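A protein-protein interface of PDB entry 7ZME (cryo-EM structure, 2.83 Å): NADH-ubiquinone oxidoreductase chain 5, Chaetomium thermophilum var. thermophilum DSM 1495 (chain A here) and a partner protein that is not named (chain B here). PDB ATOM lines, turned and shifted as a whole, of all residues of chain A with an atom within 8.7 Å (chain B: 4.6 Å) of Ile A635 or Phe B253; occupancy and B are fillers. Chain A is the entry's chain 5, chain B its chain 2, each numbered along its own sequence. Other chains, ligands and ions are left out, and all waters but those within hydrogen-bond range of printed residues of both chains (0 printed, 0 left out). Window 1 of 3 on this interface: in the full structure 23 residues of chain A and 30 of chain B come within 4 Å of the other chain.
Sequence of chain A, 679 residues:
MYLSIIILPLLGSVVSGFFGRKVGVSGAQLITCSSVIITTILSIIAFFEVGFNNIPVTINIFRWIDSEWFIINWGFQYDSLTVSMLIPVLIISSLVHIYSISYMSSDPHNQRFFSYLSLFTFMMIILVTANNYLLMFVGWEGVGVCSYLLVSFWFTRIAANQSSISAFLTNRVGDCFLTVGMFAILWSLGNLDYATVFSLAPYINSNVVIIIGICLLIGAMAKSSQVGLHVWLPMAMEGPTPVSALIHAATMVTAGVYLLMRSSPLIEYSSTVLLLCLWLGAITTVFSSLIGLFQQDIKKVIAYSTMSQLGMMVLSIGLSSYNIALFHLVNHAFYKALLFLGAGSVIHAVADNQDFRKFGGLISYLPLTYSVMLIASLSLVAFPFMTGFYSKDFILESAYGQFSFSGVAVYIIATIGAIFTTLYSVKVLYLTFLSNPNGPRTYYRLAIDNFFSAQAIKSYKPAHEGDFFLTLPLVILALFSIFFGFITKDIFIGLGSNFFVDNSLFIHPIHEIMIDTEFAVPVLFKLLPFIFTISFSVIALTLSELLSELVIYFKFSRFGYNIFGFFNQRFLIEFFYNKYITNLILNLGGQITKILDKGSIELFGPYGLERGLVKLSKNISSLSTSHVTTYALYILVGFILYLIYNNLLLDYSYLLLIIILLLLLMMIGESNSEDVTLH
O of Phe B260 is in hydrogen-bond range of NE1 of Trp B263, 3.4 Å away. The backbone carbonyl oxygen of Phe B253 lies within hydrogen-bond range of the indole nitrogen of Trp B263 (2.9 Å).
Val A628 touches Leu B182. Tyr A631 touches Leu B182. Ala A632 touches Leu B182. CD2 of Leu B182 touches CD1 of Ile A635, at 3.9 Å. CG2 of Ile A635 touches CD2 of Leu B185, 3.7 Å away. CE1 of Phe B260 touches O of Ile A635, at 3.9 Å. Phe A639 touches Phe B189 (CD1 to CE2, 3.4 Å). Phe A639 touches Ile B249. Phe A639 touches Phe B260 (N to CE1, 3.7 Å). CB of Tyr A642 touches CD1 of Ile B249 (3.7 Å).
Of chain B, only Leu B182, Leu B185, Phe B253 and Phe B260 come within 4 Å of Ile A635. Printed residues of chain B within 4 Å of Tyr A642: Ile B249. Of the printed residues of chain B, Tyr A631 touches Leu B182 (3.6 Å). Printed residues of chain A within 4 Å of Leu B185: Ile A635 (3.7 Å). Of the printed residues of chain A, Phe B260 touches Ile A635 (3.9 Å), Gly A638 (3.6 Å) and Phe A639 (3.7 Å). Leu A636 touches none of the printed residues of chain B. The nearest residue of chain A that does not touch Phe B253 is Tyr A631 (6.5 Å).
Printed residues of chain A that touch a printed residue of chain B: Val A628, Tyr A631, Ala A632, Ile A635, Gly A638, Phe A639 and Tyr A642. Hydrophobic or aromatic side chains of chain A within 4 Å of the printed part of chain B: Val A628, Tyr A631, Ala A632, Ile A635, Phe A639 and Tyr A642. Among the printed residues, no Asp or Glu carboxylate lies within 4 Å of a Lys or Arg side-chain nitrogen of the other chain.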
ATOM      1  N   VAL A 628       4.302   0.751  15.640  1.00  0.00           N
ATOM      2  CA  VAL A 628       4.883   1.019  16.988  1.00  0.00           C
ATOM      3  C   VAL A 628       4.492   2.413  17.488  1.00  0.00           C
ATOM      4  O   VAL A 628       4.291   2.565  18.692  1.00  0.00           O
ATOM      5  CB  VAL A 628       6.407   0.782  16.966  1.00  0.00           C
ATOM      6  CG1 VAL A 628       7.105   1.606  15.895  1.00  0.00           C
ATOM      7  CG2 VAL A 628       7.054   0.986  18.325  1.00  0.00           C
ATOM      8  N   THR A 629       4.412   3.392  16.591  1.00  0.00           N
ATOM      9  CA  THR A 629       4.000   4.751  17.001  1.00  0.00           C
ATOM     10  C   THR A 629       2.562   4.740  17.542  1.00  0.00           C
ATOM     11  O   THR A 629       2.315   5.425  18.546  1.00  0.00           O
ATOM     12  CB  THR A 629       4.262   5.742  15.865  1.00  0.00           C
ATOM     13  OG1 THR A 629       3.304   5.504  14.836  1.00  0.00           O
ATOM     14  CG2 THR A 629       5.664   5.623  15.309  1.00  0.00           C
ATOM     15  N   THR A 630       1.655   4.014  16.892  1.00  0.00           N
ATOM     16  CA  THR A 630       0.249   3.922  17.359  1.00  0.00           C
ATOM     17  C   THR A 630       0.232   3.195  18.695  1.00  0.00           C
ATOM     18  O   THR A 630      -0.524   3.609  19.582  1.00  0.00           O
ATOM     19  CB  THR A 630      -0.657   3.207  16.348  1.00  0.00           C
ATOM     20  OG1 THR A 630      -0.229   3.550  15.030  1.00  0.00           O
ATOM     21  CG2 THR A 630      -2.121   3.547  16.509  1.00  0.00           C
ATOM     22  N   TYR A 631       1.089   2.186  18.832  1.00  0.00           N
ATOM     23  CA  TYR A 631       1.057   1.352  20.047  1.00  0.00           C
ATOM     24  C   TYR A 631       1.757   2.125  21.157  1.00  0.00           C
ATOM     25  O   TYR A 631       1.364   1.965  22.314  1.00  0.00           O
ATOM     26  CB  TYR A 631       1.753   0.028  19.736  1.00  0.00           C
ATOM     27  CG  TYR A 631       0.945  -0.985  18.970  1.00  0.00           C
ATOM     28  CD1 TYR A 631      -0.363  -0.734  18.593  1.00  0.00           C
ATOM     29  CD2 TYR A 631       1.497  -2.209  18.631  1.00  0.00           C
ATOM     30  CE1 TYR A 631      -1.101  -1.671  17.891  1.00  0.00           C
ATOM     31  CE2 TYR A 631       0.774  -3.157  17.932  1.00  0.00           C
ATOM     32  CZ  TYR A 631      -0.530  -2.887  17.563  1.00  0.00           C
ATOM     33  OH  TYR A 631      -1.245  -3.816  16.872  1.00  0.00           O
ATOM     34  N   ALA A 632       2.757   2.936  20.817  1.00  0.00           N
ATOM     35  CA  ALA A 632       3.360   3.830  21.831  1.00  0.00           C
ATOM     36  C   ALA A 632       2.299   4.802  22.327  1.00  0.00           C
ATOM     37  O   ALA A 632       2.233   5.028  23.537  1.00  0.00           O
ATOM     38  CB  ALA A 632       4.523   4.573  21.234  1.00  0.00           C
ATOM     39  N   LEU A 633       1.517   5.363  21.406  1.00  0.00           N
ATOM     40  CA  LEU A 633       0.485   6.311  21.809  1.00  0.00           C
ATOM     41  C   LEU A 633      -0.580   5.650  22.672  1.00  0.00           C
ATOM     42  O   LEU A 633      -1.056   6.262  23.630  1.00  0.00           O
ATOM     43  CB  LEU A 633      -0.143   6.960  20.579  1.00  0.00           C
ATOM     44  CG  LEU A 633      -1.204   8.015  20.881  1.00  0.00           C
ATOM     45  CD1 LEU A 633      -0.653   9.072  21.822  1.00  0.00           C
ATOM     46  CD2 LEU A 633      -1.718   8.650  19.614  1.00  0.00           C
ATOM     47  N   TYR A 634      -0.965   4.412  22.356  1.00  0.00           N
ATOM     48  CA  TYR A 634      -1.887   3.690  23.227  1.00  0.00           C
ATOM     49  C   TYR A 634      -1.313   3.559  24.630  1.00  0.00           C
ATOM     50  O   TYR A 634      -2.020   3.773  25.620  1.00  0.00           O
ATOM     51  CB  TYR A 634      -2.190   2.302  22.660  1.00  0.00           C
ATOM     52  CG  TYR A 634      -2.943   2.273  21.351  1.00  0.00           C
ATOM     53  CD1 TYR A 634      -3.546   3.408  20.838  1.00  0.00           C
ATOM     54  CD2 TYR A 634      -3.049   1.097  20.629  1.00  0.00           C
ATOM     55  CE1 TYR A 634      -4.228   3.371  19.638  1.00  0.00           C
ATOM     56  CE2 TYR A 634      -3.728   1.048  19.436  1.00  0.00           C
ATOM     57  CZ  TYR A 634      -4.318   2.184  18.946  1.00  0.00           C
ATOM     58  OH  TYR A 634      -4.993   2.129  17.751  1.00  0.00           O
ATOM     59  N   ILE A 635      -0.027   3.211  24.729  1.00  0.00           N
ATOM     60  CA  ILE A 635       0.623   3.069  26.029  1.00  0.00           C
ATOM     61  C   ILE A 635       0.622   4.394  26.775  1.00  0.00           C
ATOM     62  O   ILE A 635       0.345   4.446  27.978  1.00  0.00           O
ATOM     63  CB  ILE A 635       2.052   2.526  25.852  1.00  0.00           C
ATOM     64  CG1 ILE A 635       2.019   1.048  25.478  1.00  0.00           C
ATOM     65  CG2 ILE A 635       2.862   2.722  27.125  1.00  0.00           C
ATOM     66  CD1 ILE A 635       3.303   0.559  24.887  1.00  0.00           C
ATOM     67  N   LEU A 636       0.933   5.486  26.075  1.00  0.00           N
ATOM     68  CA  LEU A 636       0.954   6.798  26.711  1.00  0.00           C
ATOM     69  C   LEU A 636      -0.436   7.212  27.175  1.00  0.00           C
ATOM     70  O   LEU A 636      -0.586   7.828  28.235  1.00  0.00           O
ATOM     71  CB  LEU A 636       1.531   7.834  25.747  1.00  0.00           C
ATOM     72  CG  LEU A 636       1.564   9.287  26.219  1.00  0.00           C
ATOM     73  CD1 LEU A 636       2.370   9.416  27.495  1.00  0.00           C
ATOM     74  CD2 LEU A 636       2.138  10.167  25.133  1.00  0.00           C
ATOM     75  N   VAL A 637      -1.466   6.889  26.392  1.00  0.00           N
ATOM     76  CA  VAL A 637      -2.836   7.183  26.806  1.00  0.00           C
ATOM     77  C   VAL A 637      -3.188   6.406  28.066  1.00  0.00           C
ATOM     78  O   VAL A 637      -3.746   6.956  29.022  1.00  0.00           O
ATOM     79  CB  VAL A 637      -3.818   6.872  25.664  1.00  0.00           C
ATOM     80  CG1 VAL A 637      -5.246   6.970  26.153  1.00  0.00           C
ATOM     81  CG2 VAL A 637      -3.587   7.813  24.515  1.00  0.00           C
ATOM     82  N   GLY A 638      -2.873   5.111  28.084  1.00  0.00           N
ATOM     83  CA  GLY A 638      -3.159   4.310  29.261  1.00  0.00           C
ATOM     84  C   GLY A 638      -2.331   4.722  30.460  1.00  0.00           C
ATOM     85  O   GLY A 638      -2.802   4.667  31.599  1.00  0.00           O
ATOM     86  N   PHE A 639      -1.085   5.130  30.223  1.00  0.00           N
ATOM     87  CA  PHE A 639      -0.227   5.576  31.314  1.00  0.00           C
ATOM     88  C   PHE A 639      -0.811   6.800  32.006  1.00  0.00           C
ATOM     89  O   PHE A 639      -0.971   6.818  33.231  1.00  0.00           O
ATOM     90  CB  PHE A 639       1.176   5.865  30.775  1.00  0.00           C
ATOM     91  CG  PHE A 639       2.069   6.574  31.748  1.00  0.00           C
ATOM     92  CD1 PHE A 639       2.733   5.871  32.734  1.00  0.00           C
ATOM     93  CD2 PHE A 639       2.259   7.942  31.665  1.00  0.00           C
ATOM     94  CE1 PHE A 639       3.561   6.515  33.622  1.00  0.00           C
ATOM     95  CE2 PHE A 639       3.081   8.590  32.551  1.00  0.00           C
ATOM     96  CZ  PHE A 639       3.734   7.875  33.530  1.00  0.00           C
ATOM     97  N   ILE A 640      -1.145   7.833  31.233  1.00  0.00           N
ATOM     98  CA  ILE A 640      -1.634   9.069  31.829  1.00  0.00           C
ATOM     99  C   ILE A 640      -3.017   8.876  32.431  1.00  0.00           C
ATOM    100  O   ILE A 640      -3.366   9.534  33.415  1.00  0.00           O
ATOM    101  CB  ILE A 640      -1.619  10.205  30.790  1.00  0.00           C
ATOM    102  CG1 ILE A 640      -2.549   9.888  29.623  1.00  0.00           C
ATOM    103  CG2 ILE A 640      -0.218  10.435  30.271  1.00  0.00           C
ATOM    104  CD1 ILE A 640      -2.753  11.050  28.697  1.00  0.00           C
ATOM    105  N   LEU A 641      -3.826   7.979  31.861  1.00  0.00           N
ATOM    106  CA  LEU A 641      -5.155   7.722  32.406  1.00  0.00           C
ATOM    107  C   LEU A 641      -5.072   7.093  33.791  1.00  0.00           C
ATOM    108  O   LEU A 641      -5.896   7.393  34.662  1.00  0.00           O
ATOM    109  CB  LEU A 641      -5.947   6.829  31.456  1.00  0.00           C
ATOM    110  CG  LEU A 641      -6.891   7.527  30.477  1.00  0.00           C
ATOM    111  CD1 LEU A 641      -7.522   6.519  29.548  1.00  0.00           C
ATOM    112  CD2 LEU A 641      -7.954   8.322  31.209  1.00  0.00           C
ATOM    113  N   TYR A 642      -4.098   6.207  34.005  1.00  0.00           N
ATOM    114  CA  TYR A 642      -3.890   5.642  35.335  1.00  0.00           C
ATOM    115  C   TYR A 642      -3.435   6.709  36.319  1.00  0.00           C
ATOM    116  O   TYR A 642      -3.756   6.637  37.511  1.00  0.00           O
ATOM    117  CB  TYR A 642      -2.872   4.505  35.278  1.00  0.00           C
ATOM    118  CG  TYR A 642      -3.445   3.166  34.878  1.00  0.00           C
ATOM    119  CD1 TYR A 642      -4.378   3.061  33.858  1.00  0.00           C
ATOM    120  CD2 TYR A 642      -3.042   2.005  35.512  1.00  0.00           C
ATOM    121  CE1 TYR A 642      -4.897   1.835  33.489  1.00  0.00           C
ATOM    122  CE2 TYR A 642      -3.553   0.778  35.148  1.00  0.00           C
ATOM    123  CZ  TYR A 642      -4.479   0.700  34.139  1.00  0.00           C
ATOM    124  OH  TYR A 642      -4.990  -0.517  33.775  1.00  0.00           O
ATOM    125  N   LEU B 182       8.943  -0.772  22.125  1.00  0.00           N
ATOM    126  CA  LEU B 182       7.895  -0.578  23.116  1.00  0.00           C
ATOM    127  C   LEU B 182       8.340  -1.036  24.495  1.00  0.00           C
ATOM    128  O   LEU B 182       7.864  -0.509  25.506  1.00  0.00           O
ATOM    129  CB  LEU B 182       6.633  -1.321  22.693  1.00  0.00           C
ATOM    130  CG  LEU B 182       5.777  -0.714  21.587  1.00  0.00           C
ATOM    131  CD1 LEU B 182       4.434  -1.396  21.588  1.00  0.00           C
ATOM    132  CD2 LEU B 182       5.624   0.784  21.760  1.00  0.00           C
ATOM    133  N   GLY B 183       9.238  -2.021  24.559  1.00  0.00           N
ATOM    134  CA  GLY B 183       9.825  -2.392  25.829  1.00  0.00           C
ATOM    135  C   GLY B 183      10.840  -1.403  26.354  1.00  0.00           C
ATOM    136  O   GLY B 183      11.046  -1.333  27.569  1.00  0.00           O
ATOM    137  N   LEU B 185      10.372   1.846  25.988  1.00  0.00           N
ATOM    138  CA  LEU B 185       9.447   2.769  26.633  1.00  0.00           C
ATOM    139  C   LEU B 185       8.982   2.222  27.974  1.00  0.00           C
ATOM    140  O   LEU B 185       8.753   2.982  28.920  1.00  0.00           O
ATOM    141  CB  LEU B 185       8.256   3.030  25.715  1.00  0.00           C
ATOM    142  CG  LEU B 185       7.211   4.018  26.228  1.00  0.00           C
ATOM    143  CD1 LEU B 185       7.784   5.413  26.198  1.00  0.00           C
ATOM    144  CD2 LEU B 185       5.938   3.935  25.405  1.00  0.00           C
ATOM    145  N   SER B 186       8.819   0.900  28.064  1.00  0.00           N
ATOM    146  CA  SER B 186       8.421   0.273  29.318  1.00  0.00           C
ATOM    147  C   SER B 186       9.481   0.462  30.393  1.00  0.00           C
ATOM    148  O   SER B 186       9.157   0.673  31.566  1.00  0.00           O
ATOM    149  CB  SER B 186       8.150  -1.214  29.082  1.00  0.00           C
ATOM    150  OG  SER B 186       7.789  -1.878  30.277  1.00  0.00           O
ATOM    151  N   PHE B 189       9.605   3.913  32.164  1.00  0.00           N
ATOM    152  CA  PHE B 189       8.679   4.069  33.280  1.00  0.00           C
ATOM    153  C   PHE B 189       9.225   3.408  34.539  1.00  0.00           C
ATOM    154  O   PHE B 189       9.062   3.938  35.643  1.00  0.00           O
ATOM    155  CB  PHE B 189       7.312   3.494  32.913  1.00  0.00           C
ATOM    156  CG  PHE B 189       6.566   4.304  31.889  1.00  0.00           C
ATOM    157  CD1 PHE B 189       6.988   5.573  31.544  1.00  0.00           C
ATOM    158  CD2 PHE B 189       5.439   3.792  31.269  1.00  0.00           C
ATOM    159  CE1 PHE B 189       6.300   6.316  30.601  1.00  0.00           C
ATOM    160  CE2 PHE B 189       4.750   4.532  30.325  1.00  0.00           C
ATOM    161  CZ  PHE B 189       5.179   5.793  29.995  1.00  0.00           C
ATOM    162  N   ILE B 249       3.294   0.371  36.088  1.00  0.00           N
ATOM    163  CA  ILE B 249       2.809   0.457  34.717  1.00  0.00           C
ATOM    164  C   ILE B 249       3.828  -0.131  33.753  1.00  0.00           C
ATOM    165  O   ILE B 249       3.465  -0.808  32.781  1.00  0.00           O
ATOM    166  CB  ILE B 249       2.459   1.918  34.372  1.00  0.00           C
ATOM    167  CG1 ILE B 249       1.060   2.258  34.896  1.00  0.00           C
ATOM    168  CG2 ILE B 249       2.556   2.172  32.868  1.00  0.00           C
ATOM    169  CD1 ILE B 249       0.706   3.715  34.775  1.00  0.00           C
ATOM    170  N   GLY B 250       5.117   0.100  34.009  1.00  0.00           N
ATOM    171  CA  GLY B 250       6.155  -0.482  33.182  1.00  0.00           C
ATOM    172  C   GLY B 250       6.215  -1.991  33.253  1.00  0.00           C
ATOM    173  O   GLY B 250       6.685  -2.629  32.308  1.00  0.00           O
ATOM    174  N   PHE B 251       5.749  -2.578  34.353  1.00  0.00           N
ATOM    175  CA  PHE B 251       5.691  -4.026  34.484  1.00  0.00           C
ATOM    176  C   PHE B 251       4.385  -4.617  33.976  1.00  0.00           C
ATOM    177  O   PHE B 251       4.355  -5.798  33.620  1.00  0.00           O
ATOM    178  CB  PHE B 251       5.902  -4.430  35.945  1.00  0.00           C
ATOM    179  CG  PHE B 251       7.333  -4.386  36.376  1.00  0.00           C
ATOM    180  CD1 PHE B 251       8.260  -5.248  35.826  1.00  0.00           C
ATOM    181  CD2 PHE B 251       7.759  -3.474  37.319  1.00  0.00           C
ATOM    182  CE1 PHE B 251       9.579  -5.207  36.216  1.00  0.00           C
ATOM    183  CE2 PHE B 251       9.081  -3.434  37.706  1.00  0.00           C
ATOM    184  CZ  PHE B 251       9.988  -4.301  37.157  1.00  0.00           C
ATOM    185  N   LEU B 252       3.313  -3.829  33.937  1.00  0.00           N
ATOM    186  CA  LEU B 252       2.074  -4.308  33.337  1.00  0.00           C
ATOM    187  C   LEU B 252       2.200  -4.413  31.826  1.00  0.00           C
ATOM    188  O   LEU B 252       1.526  -5.242  31.205  1.00  0.00           O
ATOM    189  CB  LEU B 252       0.916  -3.392  33.720  1.00  0.00           C
ATOM    190  CG  LEU B 252       0.486  -3.490  35.181  1.00  0.00           C
ATOM    191  CD1 LEU B 252      -0.401  -2.327  35.560  1.00  0.00           C
ATOM    192  CD2 LEU B 252      -0.222  -4.809  35.427  1.00  0.00           C
ATOM    193  N   PHE B 253       3.055  -3.587  31.220  1.00  0.00           N
ATOM    194  CA  PHE B 253       3.393  -3.777  29.816  1.00  0.00           C
ATOM    195  C   PHE B 253       4.094  -5.106  29.595  1.00  0.00           C
ATOM    196  O   PHE B 253       3.789  -5.824  28.638  1.00  0.00           O
ATOM    197  CB  PHE B 253       4.280  -2.634  29.323  1.00  0.00           C
ATOM    198  CG  PHE B 253       4.815  -2.842  27.931  1.00  0.00           C
ATOM    199  CD1 PHE B 253       6.004  -3.525  27.722  1.00  0.00           C
ATOM    200  CD2 PHE B 253       4.127  -2.368  26.834  1.00  0.00           C
ATOM    201  CE1 PHE B 253       6.487  -3.729  26.459  1.00  0.00           C
ATOM    202  CE2 PHE B 253       4.619  -2.564  25.565  1.00  0.00           C
ATOM    203  CZ  PHE B 253       5.794  -3.249  25.382  1.00  0.00           C
ATOM    204  N   LYS B 254       5.119  -5.357  30.399  1.00  0.00           N
ATOM    205  CA  LYS B 254       5.980  -6.542  30.192  1.00  0.00           C
ATOM    206  C   LYS B 254       5.194  -7.841  30.353  1.00  0.00           C
ATOM    207  O   LYS B 254       5.491  -8.799  29.632  1.00  0.00           O
ATOM    208  CB  LYS B 254       7.196  -6.416  31.110  1.00  0.00           C
ATOM    209  CG  LYS B 254       8.098  -5.223  30.845  1.00  0.00           C
ATOM    210  CD  LYS B 254       9.432  -5.338  31.537  1.00  0.00           C
ATOM    211  CE  LYS B 254      10.317  -4.124  31.354  1.00  0.00           C
ATOM    212  NZ  LYS B 254      10.535  -3.794  29.930  1.00  0.00           N
ATOM    213  N   VAL B 255       4.220  -7.873  31.262  1.00  0.00           N
ATOM    214  CA  VAL B 255       3.367  -9.087  31.416  1.00  0.00           C
ATOM    215  C   VAL B 255       2.247  -9.044  30.390  1.00  0.00           C
ATOM    216  O   VAL B 255       1.525 -10.039  30.315  1.00  0.00           O
ATOM    217  CB  VAL B 255       2.837  -9.278  32.844  1.00  0.00           C
ATOM    218  CG1 VAL B 255       3.961  -9.595  33.818  1.00  0.00           C
ATOM    219  CG2 VAL B 255       1.993  -8.107  33.322  1.00  0.00           C
ATOM    220  N   SER B 256       2.062  -7.915  29.718  1.00  0.00           N
ATOM    221  CA  SER B 256       1.053  -7.754  28.644  1.00  0.00           C
ATOM    222  C   SER B 256      -0.347  -7.651  29.244  1.00  0.00           C
ATOM    223  O   SER B 256      -1.247  -8.314  28.732  1.00  0.00           O
ATOM    224  CB  SER B 256       1.180  -8.767  27.560  1.00  0.00           C
ATOM    225  OG  SER B 256       0.349  -8.421  26.469  1.00  0.00           O
ATOM    226  N   PHE B 260      -2.102  -2.227  28.187  1.00  0.00           N
ATOM    227  CA  PHE B 260      -0.736  -2.180  27.681  1.00  0.00           C
ATOM    228  C   PHE B 260      -0.378  -3.501  27.021  1.00  0.00           C
ATOM    229  O   PHE B 260       0.718  -4.032  27.192  1.00  0.00           O
ATOM    230  CB  PHE B 260       0.248  -1.845  28.797  1.00  0.00           C
ATOM    231  CG  PHE B 260      -0.261  -0.817  29.757  1.00  0.00           C
ATOM    232  CD1 PHE B 260      -0.193   0.529  29.448  1.00  0.00           C
ATOM    233  CD2 PHE B 260      -0.823  -1.197  30.963  1.00  0.00           C
ATOM    234  CE1 PHE B 260      -0.668   1.476  30.328  1.00  0.00           C
ATOM    235  CE2 PHE B 260      -1.299  -0.254  31.844  1.00  0.00           C
ATOM    236  CZ  PHE B 260      -1.224   1.085  31.528  1.00  0.00           C
ATOM    237  N   TRP B 263       0.931  -5.015  21.931  1.00  0.00           N
ATOM    238  CA  TRP B 263       2.203  -5.533  21.374  1.00  0.00           C
ATOM    239  C   TRP B 263       2.253  -7.054  21.298  1.00  0.00           C
ATOM    240  O   TRP B 263       2.653  -7.560  20.262  1.00  0.00           O
ATOM    241  CB  TRP B 263       3.355  -4.980  22.223  1.00  0.00           C
ATOM    242  CG  TRP B 263       3.486  -5.566  23.593  1.00  0.00           C
ATOM    243  CD1 TRP B 263       2.865  -5.144  24.729  1.00  0.00           C
ATOM    244  CD2 TRP B 263       4.288  -6.697  23.969  1.00  0.00           C
ATOM    245  NE1 TRP B 263       3.228  -5.932  25.786  1.00  0.00           N
ATOM    246  CE2 TRP B 263       4.094  -6.898  25.350  1.00  0.00           C
ATOM    247  CE3 TRP B 263       5.133  -7.567  23.271  1.00  0.00           C
ATOM    248  CZ2 TRP B 263       4.727  -7.924  26.047  1.00  0.00           C
ATOM    249  CZ3 TRP B 263       5.735  -8.597  23.956  1.00  0.00           C
ATOM    250  CH2 TRP B 263       5.542  -8.763  25.327  1.00  0.00           C
